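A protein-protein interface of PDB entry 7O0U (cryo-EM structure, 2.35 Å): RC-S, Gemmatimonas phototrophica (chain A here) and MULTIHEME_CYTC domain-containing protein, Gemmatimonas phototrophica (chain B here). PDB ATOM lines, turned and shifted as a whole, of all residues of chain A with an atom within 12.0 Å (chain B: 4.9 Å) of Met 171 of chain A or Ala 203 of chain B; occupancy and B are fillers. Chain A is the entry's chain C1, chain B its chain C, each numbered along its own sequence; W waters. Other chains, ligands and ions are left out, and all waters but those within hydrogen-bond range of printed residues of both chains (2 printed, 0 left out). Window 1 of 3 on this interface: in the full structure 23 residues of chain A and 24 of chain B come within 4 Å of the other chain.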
ATOM      1  N   ARG A 165     -16.050 -18.788   5.669  1.00  0.00           N
ATOM      2  CA  ARG A 165     -14.692 -19.310   5.769  1.00  0.00           C
ATOM      3  C   ARG A 165     -14.488 -20.018   7.103  1.00  0.00           C
ATOM      4  O   ARG A 165     -14.934 -19.542   8.149  1.00  0.00           O
ATOM      5  CB  ARG A 165     -13.681 -18.171   5.640  1.00  0.00           C
ATOM      6  CG  ARG A 165     -13.535 -17.583   4.248  1.00  0.00           C
ATOM      7  CD  ARG A 165     -12.480 -16.487   4.246  1.00  0.00           C
ATOM      8  NE  ARG A 165     -12.245 -15.939   2.916  1.00  0.00           N
ATOM      9  CZ  ARG A 165     -11.469 -14.893   2.664  1.00  0.00           C
ATOM     10  NH1 ARG A 165     -10.772 -14.302   3.620  1.00  0.00           N
ATOM     11  NH2 ARG A 165     -11.377 -14.440   1.418  1.00  0.00           N
ATOM     12  N   ARG A 166     -13.797 -21.163   7.069  1.00  0.00           N
ATOM     13  CA  ARG A 166     -13.330 -21.764   8.317  1.00  0.00           C
ATOM     14  C   ARG A 166     -12.169 -20.997   8.939  1.00  0.00           C
ATOM     15  O   ARG A 166     -12.036 -20.977  10.167  1.00  0.00           O
ATOM     16  CB  ARG A 166     -12.901 -23.216   8.099  1.00  0.00           C
ATOM     17  CG  ARG A 166     -13.989 -24.187   7.687  1.00  0.00           C
ATOM     18  CD  ARG A 166     -13.505 -25.610   7.932  1.00  0.00           C
ATOM     19  NE  ARG A 166     -14.214 -26.606   7.142  1.00  0.00           N
ATOM     20  CZ  ARG A 166     -14.811 -27.679   7.643  1.00  0.00           C
ATOM     21  NH1 ARG A 166     -15.104 -27.768   8.929  1.00  0.00           N
ATOM     22  NH2 ARG A 166     -15.199 -28.647   6.820  1.00  0.00           N
ATOM     23  N   MET A 167     -11.322 -20.371   8.128  1.00  0.00           N
ATOM     24  CA  MET A 167     -10.142 -19.671   8.623  1.00  0.00           C
ATOM     25  C   MET A 167     -10.439 -18.185   8.781  1.00  0.00           C
ATOM     26  O   MET A 167     -10.715 -17.492   7.796  1.00  0.00           O
ATOM     27  CB  MET A 167      -8.953 -19.905   7.695  1.00  0.00           C
ATOM     28  CG  MET A 167      -8.437 -21.334   7.787  1.00  0.00           C
ATOM     29  SD  MET A 167      -7.021 -21.689   6.743  1.00  0.00           S
ATOM     30  CE  MET A 167      -5.769 -20.746   7.600  1.00  0.00           C
ATOM     31  N   ARG A 168     -10.371 -17.700  10.021  1.00  0.00           N
ATOM     32  CA  ARG A 168     -10.695 -16.315  10.333  1.00  0.00           C
ATOM     33  C   ARG A 168      -9.526 -15.355  10.128  1.00  0.00           C
ATOM     34  O   ARG A 168      -9.727 -14.140  10.226  1.00  0.00           O
ATOM     35  CB  ARG A 168     -11.239 -16.230  11.761  1.00  0.00           C
ATOM     36  CG  ARG A 168     -12.629 -16.854  11.863  1.00  0.00           C
ATOM     37  CD  ARG A 168     -13.265 -16.748  13.238  1.00  0.00           C
ATOM     38  NE  ARG A 168     -13.477 -15.363  13.636  1.00  0.00           N
ATOM     39  CZ  ARG A 168     -12.797 -14.738  14.587  1.00  0.00           C
ATOM     40  NH1 ARG A 168     -11.920 -15.376  15.342  1.00  0.00           N
ATOM     41  NH2 ARG A 168     -13.023 -13.447  14.802  1.00  0.00           N
ATOM     42  N   GLY A 169      -8.320 -15.860   9.866  1.00  0.00           N
ATOM     43  CA  GLY A 169      -7.152 -15.022   9.644  1.00  0.00           C
ATOM     44  C   GLY A 169      -7.324 -14.086   8.463  1.00  0.00           C
ATOM     45  O   GLY A 169      -7.778 -14.507   7.397  1.00  0.00           O
ATOM     46  N   ILE A 170      -6.976 -12.810   8.639  1.00  0.00           N
ATOM     47  CA  ILE A 170      -7.436 -11.784   7.707  1.00  0.00           C
ATOM     48  C   ILE A 170      -6.652 -11.765   6.391  1.00  0.00           C
ATOM     49  O   ILE A 170      -7.223 -11.461   5.339  1.00  0.00           O
ATOM     50  CB  ILE A 170      -7.384 -10.407   8.394  1.00  0.00           C
ATOM     51  CG1 ILE A 170      -8.122 -10.435   9.735  1.00  0.00           C
ATOM     52  CG2 ILE A 170      -7.987  -9.337   7.501  1.00  0.00           C
ATOM     53  CD1 ILE A 170      -9.586 -10.788   9.628  1.00  0.00           C
ATOM     54  N   MET A 171      -5.361 -12.096   6.398  1.00  0.00           N
ATOM     55  CA  MET A 171      -4.552 -12.024   5.182  1.00  0.00           C
ATOM     56  C   MET A 171      -4.473 -13.335   4.405  1.00  0.00           C
ATOM     57  O   MET A 171      -3.839 -13.367   3.345  1.00  0.00           O
ATOM     58  CB  MET A 171      -3.135 -11.541   5.510  1.00  0.00           C
ATOM     59  CG  MET A 171      -3.081 -10.123   6.053  1.00  0.00           C
ATOM     60  SD  MET A 171      -1.407  -9.473   6.165  1.00  0.00           S
ATOM     61  CE  MET A 171      -0.966  -9.395   4.433  1.00  0.00           C
ATOM     62  N   ILE A 172      -5.092 -14.402   4.912  1.00  0.00           N
ATOM     63  CA  ILE A 172      -4.894 -15.759   4.393  1.00  0.00           C
ATOM     64  C   ILE A 172      -5.113 -15.856   2.882  1.00  0.00           C
ATOM     65  O   ILE A 172      -4.432 -16.627   2.194  1.00  0.00           O
ATOM     66  CB  ILE A 172      -5.788 -16.749   5.165  1.00  0.00           C
ATOM     67  CG1 ILE A 172      -5.301 -18.177   4.934  1.00  0.00           C
ATOM     68  CG2 ILE A 172      -7.259 -16.583   4.795  1.00  0.00           C
ATOM     69  CD1 ILE A 172      -3.993 -18.470   5.619  1.00  0.00           C
ATOM     70  N   GLN A 173      -6.057 -15.084   2.342  1.00  0.00           N
ATOM     71  CA  GLN A 173      -6.309 -15.107   0.902  1.00  0.00           C
ATOM     72  C   GLN A 173      -5.087 -14.676   0.095  1.00  0.00           C
ATOM     73  O   GLN A 173      -4.792 -15.260  -0.953  1.00  0.00           O
ATOM     74  CB  GLN A 173      -7.516 -14.229   0.571  1.00  0.00           C
ATOM     75  CG  GLN A 173      -7.938 -14.251  -0.889  1.00  0.00           C
ATOM     76  CD  GLN A 173      -9.121 -13.340  -1.163  1.00  0.00           C
ATOM     77  OE1 GLN A 173      -9.692 -12.754  -0.245  1.00  0.00           O
ATOM     78  NE2 GLN A 173      -9.493 -13.218  -2.430  1.00  0.00           N
ATOM     79  N   SER A 174      -4.360 -13.665   0.565  1.00  0.00           N
ATOM     80  CA  SER A 174      -3.149 -13.244  -0.135  1.00  0.00           C
ATOM     81  C   SER A 174      -1.924 -14.071   0.249  1.00  0.00           C
ATOM     82  O   SER A 174      -1.121 -14.423  -0.621  1.00  0.00           O
ATOM     83  CB  SER A 174      -2.889 -11.760   0.122  1.00  0.00           C
ATOM     84  OG  SER A 174      -2.525 -11.535   1.469  1.00  0.00           O
ATOM     85  N   THR A 175      -1.755 -14.394   1.533  1.00  0.00           N
ATOM     86  CA  THR A 175      -0.510 -15.017   1.976  1.00  0.00           C
ATOM     87  C   THR A 175      -0.448 -16.519   1.712  1.00  0.00           C
ATOM     88  O   THR A 175       0.654 -17.064   1.585  1.00  0.00           O
ATOM     89  CB  THR A 175      -0.286 -14.753   3.467  1.00  0.00           C
ATOM     90  OG1 THR A 175      -1.422 -15.203   4.214  1.00  0.00           O
ATOM     91  CG2 THR A 175      -0.071 -13.269   3.719  1.00  0.00           C
ATOM     92  N   LEU A 176      -1.587 -17.209   1.626  1.00  0.00           N
ATOM     93  CA  LEU A 176      -1.583 -18.651   1.388  1.00  0.00           C
ATOM     94  C   LEU A 176      -2.367 -19.045   0.142  1.00  0.00           C
ATOM     95  O   LEU A 176      -1.801 -19.675  -0.756  1.00  0.00           O
ATOM     96  CB  LEU A 176      -2.125 -19.390   2.617  1.00  0.00           C
ATOM     97  CG  LEU A 176      -2.216 -20.915   2.501  1.00  0.00           C
ATOM     98  CD1 LEU A 176      -0.838 -21.531   2.384  1.00  0.00           C
ATOM     99  CD2 LEU A 176      -2.955 -21.500   3.688  1.00  0.00           C
ATOM    100  N   TRP A 177      -3.655 -18.705   0.062  1.00  0.00           N
ATOM    101  CA  TRP A 177      -4.516 -19.236  -0.990  1.00  0.00           C
ATOM    102  C   TRP A 177      -4.139 -18.726  -2.375  1.00  0.00           C
ATOM    103  O   TRP A 177      -4.489 -19.365  -3.372  1.00  0.00           O
ATOM    104  CB  TRP A 177      -5.981 -18.891  -0.722  1.00  0.00           C
ATOM    105  CG  TRP A 177      -6.531 -19.399   0.573  1.00  0.00           C
ATOM    106  CD1 TRP A 177      -5.947 -20.289   1.425  1.00  0.00           C
ATOM    107  CD2 TRP A 177      -7.810 -19.085   1.134  1.00  0.00           C
ATOM    108  NE1 TRP A 177      -6.771 -20.525   2.498  1.00  0.00           N
ATOM    109  CE2 TRP A 177      -7.923 -19.801   2.341  1.00  0.00           C
ATOM    110  CE3 TRP A 177      -8.868 -18.263   0.737  1.00  0.00           C
ATOM    111  CZ2 TRP A 177      -9.051 -19.718   3.154  1.00  0.00           C
ATOM    112  CZ3 TRP A 177      -9.985 -18.180   1.545  1.00  0.00           C
ATOM    113  CH2 TRP A 177     -10.069 -18.904   2.739  1.00  0.00           C
ATOM    114  N   ASP A 178      -3.440 -17.595  -2.457  1.00  0.00           N
ATOM    115  CA  ASP A 178      -2.951 -17.102  -3.739  1.00  0.00           C
ATOM    116  C   ASP A 178      -1.944 -18.044  -4.386  1.00  0.00           C
ATOM    117  O   ASP A 178      -1.770 -17.999  -5.608  1.00  0.00           O
ATOM    118  CB  ASP A 178      -2.325 -15.720  -3.533  1.00  0.00           C
ATOM    119  CG  ASP A 178      -2.539 -14.795  -4.712  1.00  0.00           C
ATOM    120  OD1 ASP A 178      -3.319 -15.149  -5.619  1.00  0.00           O
ATOM    121  OD2 ASP A 178      -1.936 -13.701  -4.719  1.00  0.00           O
ATOM    122  N   MET A 179      -1.280 -18.892  -3.607  1.00  0.00           N
ATOM    123  CA  MET A 179      -0.327 -19.859  -4.134  1.00  0.00           C
ATOM    124  C   MET A 179      -0.705 -21.313  -3.877  1.00  0.00           C
ATOM    125  O   MET A 179      -0.297 -22.184  -4.648  1.00  0.00           O
ATOM    126  CB  MET A 179       1.077 -19.564  -3.580  1.00  0.00           C
ATOM    127  CG  MET A 179       1.284 -19.868  -2.109  1.00  0.00           C
ATOM    128  SD  MET A 179       2.957 -19.429  -1.598  1.00  0.00           S
ATOM    129  CE  MET A 179       2.880 -19.735   0.162  1.00  0.00           C
ATOM    130  N   ASP A 180      -1.458 -21.598  -2.817  1.00  0.00           N
ATOM    131  CA  ASP A 180      -1.921 -22.950  -2.516  1.00  0.00           C
ATOM    132  C   ASP A 180      -3.169 -23.286  -3.327  1.00  0.00           C
ATOM    133  O   ASP A 180      -4.220 -22.665  -3.141  1.00  0.00           O
ATOM    134  CB  ASP A 180      -2.212 -23.072  -1.023  1.00  0.00           C
ATOM    135  CG  ASP A 180      -2.616 -24.470  -0.620  1.00  0.00           C
ATOM    136  OD1 ASP A 180      -2.217 -25.432  -1.308  1.00  0.00           O
ATOM    137  OD2 ASP A 180      -3.341 -24.609   0.386  1.00  0.00           O
ATOM    138  N   ARG A 189     -11.583 -24.985   2.826  1.00  0.00           N
ATOM    139  CA  ARG A 189     -11.619 -23.556   3.134  1.00  0.00           C
ATOM    140  C   ARG A 189     -12.995 -23.081   3.589  1.00  0.00           C
ATOM    141  O   ARG A 189     -13.092 -22.083   4.310  1.00  0.00           O
ATOM    142  CB  ARG A 189     -11.172 -22.755   1.913  1.00  0.00           C
ATOM    143  CG  ARG A 189      -9.710 -22.935   1.573  1.00  0.00           C
ATOM    144  CD  ARG A 189      -9.353 -22.269   0.261  1.00  0.00           C
ATOM    145  NE  ARG A 189      -7.987 -22.590  -0.133  1.00  0.00           N
ATOM    146  CZ  ARG A 189      -7.437 -22.250  -1.290  1.00  0.00           C
ATOM    147  NH1 ARG A 189      -8.121 -21.601  -2.217  1.00  0.00           N
ATOM    148  NH2 ARG A 189      -6.170 -22.576  -1.525  1.00  0.00           N
ATOM    149  N   TYR A 190     -14.060 -23.759   3.180  1.00  0.00           N
ATOM    150  CA  TYR A 190     -15.417 -23.356   3.516  1.00  0.00           C
ATOM    151  C   TYR A 190     -16.122 -24.476   4.269  1.00  0.00           C
ATOM    152  O   TYR A 190     -15.811 -25.656   4.090  1.00  0.00           O
ATOM    153  CB  TYR A 190     -16.179 -22.947   2.254  1.00  0.00           C
ATOM    154  CG  TYR A 190     -15.593 -21.692   1.654  1.00  0.00           C
ATOM    155  CD1 TYR A 190     -15.970 -20.439   2.115  1.00  0.00           C
ATOM    156  CD2 TYR A 190     -14.609 -21.761   0.679  1.00  0.00           C
ATOM    157  CE1 TYR A 190     -15.434 -19.290   1.576  1.00  0.00           C
ATOM    158  CE2 TYR A 190     -14.050 -20.616   0.147  1.00  0.00           C
ATOM    159  CZ  TYR A 190     -14.469 -19.384   0.597  1.00  0.00           C
ATOM    160  OH  TYR A 190     -13.903 -18.241   0.084  1.00  0.00           O
ATOM    161  N   TYR B 168     -11.331  -9.764  -0.856  1.00  0.00           N
ATOM    162  CA  TYR B 168     -10.845  -8.419  -1.157  1.00  0.00           C
ATOM    163  C   TYR B 168     -11.108  -7.993  -2.598  1.00  0.00           C
ATOM    164  O   TYR B 168     -11.103  -6.793  -2.881  1.00  0.00           O
ATOM    165  CB  TYR B 168      -9.350  -8.288  -0.813  1.00  0.00           C
ATOM    166  CG  TYR B 168      -8.386  -9.213  -1.538  1.00  0.00           C
ATOM    167  CD1 TYR B 168      -8.189  -9.130  -2.910  1.00  0.00           C
ATOM    168  CD2 TYR B 168      -7.640 -10.146  -0.830  1.00  0.00           C
ATOM    169  CE1 TYR B 168      -7.307  -9.971  -3.557  1.00  0.00           C
ATOM    170  CE2 TYR B 168      -6.750 -10.984  -1.468  1.00  0.00           C
ATOM    171  CZ  TYR B 168      -6.588 -10.894  -2.831  1.00  0.00           C
ATOM    172  OH  TYR B 168      -5.704 -11.731  -3.468  1.00  0.00           O
ATOM    173  N   GLU B 199      -4.983  -5.159   8.019  1.00  0.00           N
ATOM    174  CA  GLU B 199      -4.663  -6.461   7.434  1.00  0.00           C
ATOM    175  C   GLU B 199      -5.412  -6.714   6.129  1.00  0.00           C
ATOM    176  O   GLU B 199      -4.856  -7.300   5.194  1.00  0.00           O
ATOM    177  CB  GLU B 199      -4.964  -7.588   8.425  1.00  0.00           C
ATOM    178  CG  GLU B 199      -4.016  -7.683   9.597  1.00  0.00           C
ATOM    179  CD  GLU B 199      -4.396  -8.775  10.575  1.00  0.00           C
ATOM    180  OE1 GLU B 199      -4.098  -9.953  10.294  1.00  0.00           O
ATOM    181  OE2 GLU B 199      -4.988  -8.458  11.628  1.00  0.00           O
ATOM    182  N   TRP B 200      -6.670  -6.280   6.043  1.00  0.00           N
ATOM    183  CA  TRP B 200      -7.427  -6.443   4.803  1.00  0.00           C
ATOM    184  C   TRP B 200      -6.879  -5.578   3.674  1.00  0.00           C
ATOM    185  O   TRP B 200      -6.762  -6.042   2.536  1.00  0.00           O
ATOM    186  CB  TRP B 200      -8.899  -6.125   5.055  1.00  0.00           C
ATOM    187  CG  TRP B 200      -9.800  -6.350   3.880  1.00  0.00           C
ATOM    188  CD1 TRP B 200     -10.498  -7.485   3.596  1.00  0.00           C
ATOM    189  CD2 TRP B 200     -10.125  -5.410   2.848  1.00  0.00           C
ATOM    190  NE1 TRP B 200     -11.226  -7.318   2.446  1.00  0.00           N
ATOM    191  CE2 TRP B 200     -11.016  -6.051   1.967  1.00  0.00           C
ATOM    192  CE3 TRP B 200      -9.744  -4.092   2.580  1.00  0.00           C
ATOM    193  CZ2 TRP B 200     -11.532  -5.421   0.838  1.00  0.00           C
ATOM    194  CZ3 TRP B 200     -10.257  -3.469   1.458  1.00  0.00           C
ATOM    195  CH2 TRP B 200     -11.142  -4.133   0.602  1.00  0.00           C
ATOM    196  N   THR B 201      -6.548  -4.319   3.964  1.00  0.00           N
ATOM    197  CA  THR B 201      -5.885  -3.481   2.968  1.00  0.00           C
ATOM    198  C   THR B 201      -4.549  -4.077   2.543  1.00  0.00           C
ATOM    199  O   THR B 201      -4.200  -4.057   1.358  1.00  0.00           O
ATOM    200  CB  THR B 201      -5.699  -2.064   3.514  1.00  0.00           C
ATOM    201  OG1 THR B 201      -6.981  -1.482   3.771  1.00  0.00           O
ATOM    202  CG2 THR B 201      -4.962  -1.191   2.510  1.00  0.00           C
ATOM    203  N   TYR B 202      -3.793  -4.621   3.498  1.00  0.00           N
ATOM    204  CA  TYR B 202      -2.501  -5.221   3.186  1.00  0.00           C
ATOM    205  C   TYR B 202      -2.652  -6.420   2.253  1.00  0.00           C
ATOM    206  O   TYR B 202      -1.879  -6.572   1.301  1.00  0.00           O
ATOM    207  CB  TYR B 202      -1.823  -5.619   4.502  1.00  0.00           C
ATOM    208  CG  TYR B 202      -0.344  -5.932   4.457  1.00  0.00           C
ATOM    209  CD1 TYR B 202       0.398  -5.787   3.296  1.00  0.00           C
ATOM    210  CD2 TYR B 202       0.321  -6.327   5.609  1.00  0.00           C
ATOM    211  CE1 TYR B 202       1.750  -6.081   3.273  1.00  0.00           C
ATOM    212  CE2 TYR B 202       1.669  -6.604   5.600  1.00  0.00           C
ATOM    213  CZ  TYR B 202       2.380  -6.481   4.431  1.00  0.00           C
ATOM    214  OH  TYR B 202       3.729  -6.741   4.429  1.00  0.00           O
ATOM    215  N   ALA B 203      -3.645  -7.278   2.505  1.00  0.00           N
ATOM    216  CA  ALA B 203      -3.943  -8.383   1.597  1.00  0.00           C
ATOM    217  C   ALA B 203      -4.284  -7.892   0.191  1.00  0.00           C
ATOM    218  O   ALA B 203      -3.777  -8.419  -0.805  1.00  0.00           O
ATOM    219  CB  ALA B 203      -5.085  -9.226   2.162  1.00  0.00           C
ATOM    220  N   LEU B 204      -5.159  -6.889   0.098  1.00  0.00           N
ATOM    221  CA  LEU B 204      -5.514  -6.288  -1.186  1.00  0.00           C
ATOM    222  C   LEU B 204      -4.296  -5.749  -1.930  1.00  0.00           C
ATOM    223  O   LEU B 204      -4.174  -5.931  -3.147  1.00  0.00           O
ATOM    224  CB  LEU B 204      -6.535  -5.174  -0.960  1.00  0.00           C
ATOM    225  CG  LEU B 204      -6.930  -4.286  -2.140  1.00  0.00           C
ATOM    226  CD1 LEU B 204      -7.749  -5.063  -3.154  1.00  0.00           C
ATOM    227  CD2 LEU B 204      -7.691  -3.070  -1.647  1.00  0.00           C
ATOM    228  N   MET B 205      -3.390  -5.081  -1.219  1.00  0.00           N
ATOM    229  CA  MET B 205      -2.235  -4.450  -1.851  1.00  0.00           C
ATOM    230  C   MET B 205      -1.198  -5.459  -2.332  1.00  0.00           C
ATOM    231  O   MET B 205      -0.543  -5.226  -3.353  1.00  0.00           O
ATOM    232  CB  MET B 205      -1.613  -3.456  -0.873  1.00  0.00           C
ATOM    233  CG  MET B 205      -2.472  -2.228  -0.658  1.00  0.00           C
ATOM    234  SD  MET B 205      -2.618  -1.237  -2.157  1.00  0.00           S
ATOM    235  CE  MET B 205      -4.302  -0.660  -1.985  1.00  0.00           C
ATOM    236  N   ILE B 206      -1.036  -6.575  -1.624  1.00  0.00           N
ATOM    237  CA  ILE B 206      -0.220  -7.675  -2.134  1.00  0.00           C
ATOM    238  C   ILE B 206      -0.765  -8.199  -3.459  1.00  0.00           C
ATOM    239  O   ILE B 206      -0.002  -8.469  -4.394  1.00  0.00           O
ATOM    240  CB  ILE B 206      -0.116  -8.789  -1.075  1.00  0.00           C
ATOM    241  CG1 ILE B 206       0.766  -8.326   0.083  1.00  0.00           C
ATOM    242  CG2 ILE B 206       0.437 -10.066  -1.680  1.00  0.00           C
ATOM    243  CD1 ILE B 206       0.768  -9.259   1.264  1.00  0.00           C
ATOM    244  N   SER B 207      -2.086  -8.340  -3.567  1.00  0.00           N
ATOM    245  CA  SER B 207      -2.697  -8.739  -4.834  1.00  0.00           C
ATOM    246  C   SER B 207      -2.373  -7.768  -5.966  1.00  0.00           C
ATOM    247  O   SER B 207      -2.027  -8.188  -7.075  1.00  0.00           O
ATOM    248  CB  SER B 207      -4.210  -8.860  -4.659  1.00  0.00           C
ATOM    249  OG  SER B 207      -4.816  -9.383  -5.826  1.00  0.00           O
HETATM  250  O   HOH W   1      -5.072 -12.244  10.931  1.00  0.00           O
HETATM  251  O   HOH W   2      -2.744 -11.680  -3.184  1.00  0.00           O
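Water W1 bridges the side-chain carboxylate of Glu 199 of chain B (2.6 Å) and the backbone NH of Ile 170 of chain A (3.0 Å).
Water W2 lies within hydrogen-bond range of the side-chain carboxylate (OD2) of Asp 178 of chain A, the side-chain hydroxyl (OH) of Tyr 168 of chain B and the backbone NH (N) of Ser 207 of chain B.
Ile 170 of chain A touches Glu 199 of chain B (CG2 to CB, 3.6 Å).
Ile 170 of chain A touches Trp 200 of chain B (CG2 to N, 3.6 Å).
CG of Met 171 of chain A touches O of Glu 199 of chain B, 3.4 Å away.
Tyr 202 of chain B touches Met 171 of chain A (CG to CE, 3.5 Å).
N of Ala 203 of chain B touches CE of Met 171 of chain A (3.9 Å).
Ile 206 of chain B touches Met 171 of chain A (CD1 to CE, 3.6 Å).
Ala 203 of chain B touches Ser 174 of chain A (CA to OG, 3.5 Å).
Of the 18 printed residues of chain A, 4 touch a printed residue of chain B.
Hydrophobic or aromatic side chains of chain A within 4 Å of the printed part of chain B: Ile 170 and Met 171.
Printed residues of chain B that touch a printed residue of chain A: Tyr 168, Glu 199, Trp 200, Tyr 202, Ala 203 and Ile 206.
OE1 of Gln 173 of chain A sits close to N of Tyr 168 of chain B, 3.5 Å away.
OH of Tyr 168 of chain B sits close to OG of Ser 207 of chain B.
The guanidinium group of Arg 165 of chain A lies within hydrogen-bond range of the side-chain amide oxygen of Gln 173 of chain A, at 2.9 Å.
The backbone carbonyl oxygen (O) of Met 171 of chain A sits at hydrogen-bond distance from the side-chain hydroxyl (OG) of Ser 174 of chain A (2.9 Å).
OG1 of Thr 175 of chain A lies within hydrogen-bond range of O of Met 171 of chain A.
The backbone carbonyl oxygen (O) of Gln 173 of chain A is in hydrogen-bond range of the backbone NH (N) of Asp 178 of chain A.
Of the printed residues of chain B, Met 171 of chain A touches Glu 199 (3.4 Å), Tyr 202 (3.5 Å), Ala 203 (3.9 Å) and Ile 206 (3.6 Å).
Ala 203 of chain B touches just these residues of chain A: Met 171 (3.9 Å) and Ser 174 (3.5 Å).
Of chain A, only Gln 173 (3.4 Å) comes within 4 Å of Tyr 168 of chain B.
Trp 200 of chain B touches one residue of chain A.
Of chain A, only Met 171 (3.5 Å) comes within 4 Å of Tyr 202 of chain B.
No residue of chain A comes within 4 Å of Leu 204 of chain B.
No residue of chain A comes within 4 Å of Met 205 of chain B.
No residue of chain A comes within 4 Å of Ser 207 of chain B.
Of the printed residues of chain B, Ser 174 of chain A touches Ala 203 (3.5 Å).
Printed residues of chain B within 4 Å of Gln 173 of chain A: Tyr 168 (3.4 Å).
Of the printed residues of chain B, Ile 170 of chain A touches Glu 199 (3.6 Å) and Trp 200 (3.6 Å).
Tyr 190 of chain A touches none of the printed residues of chain B.
Arg 189 of chain A touches none of the printed residues of chain B.
The nearest residue of chain A that does not touch Ala 203 of chain B is Ile 170 of chain A (4.4 Å).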
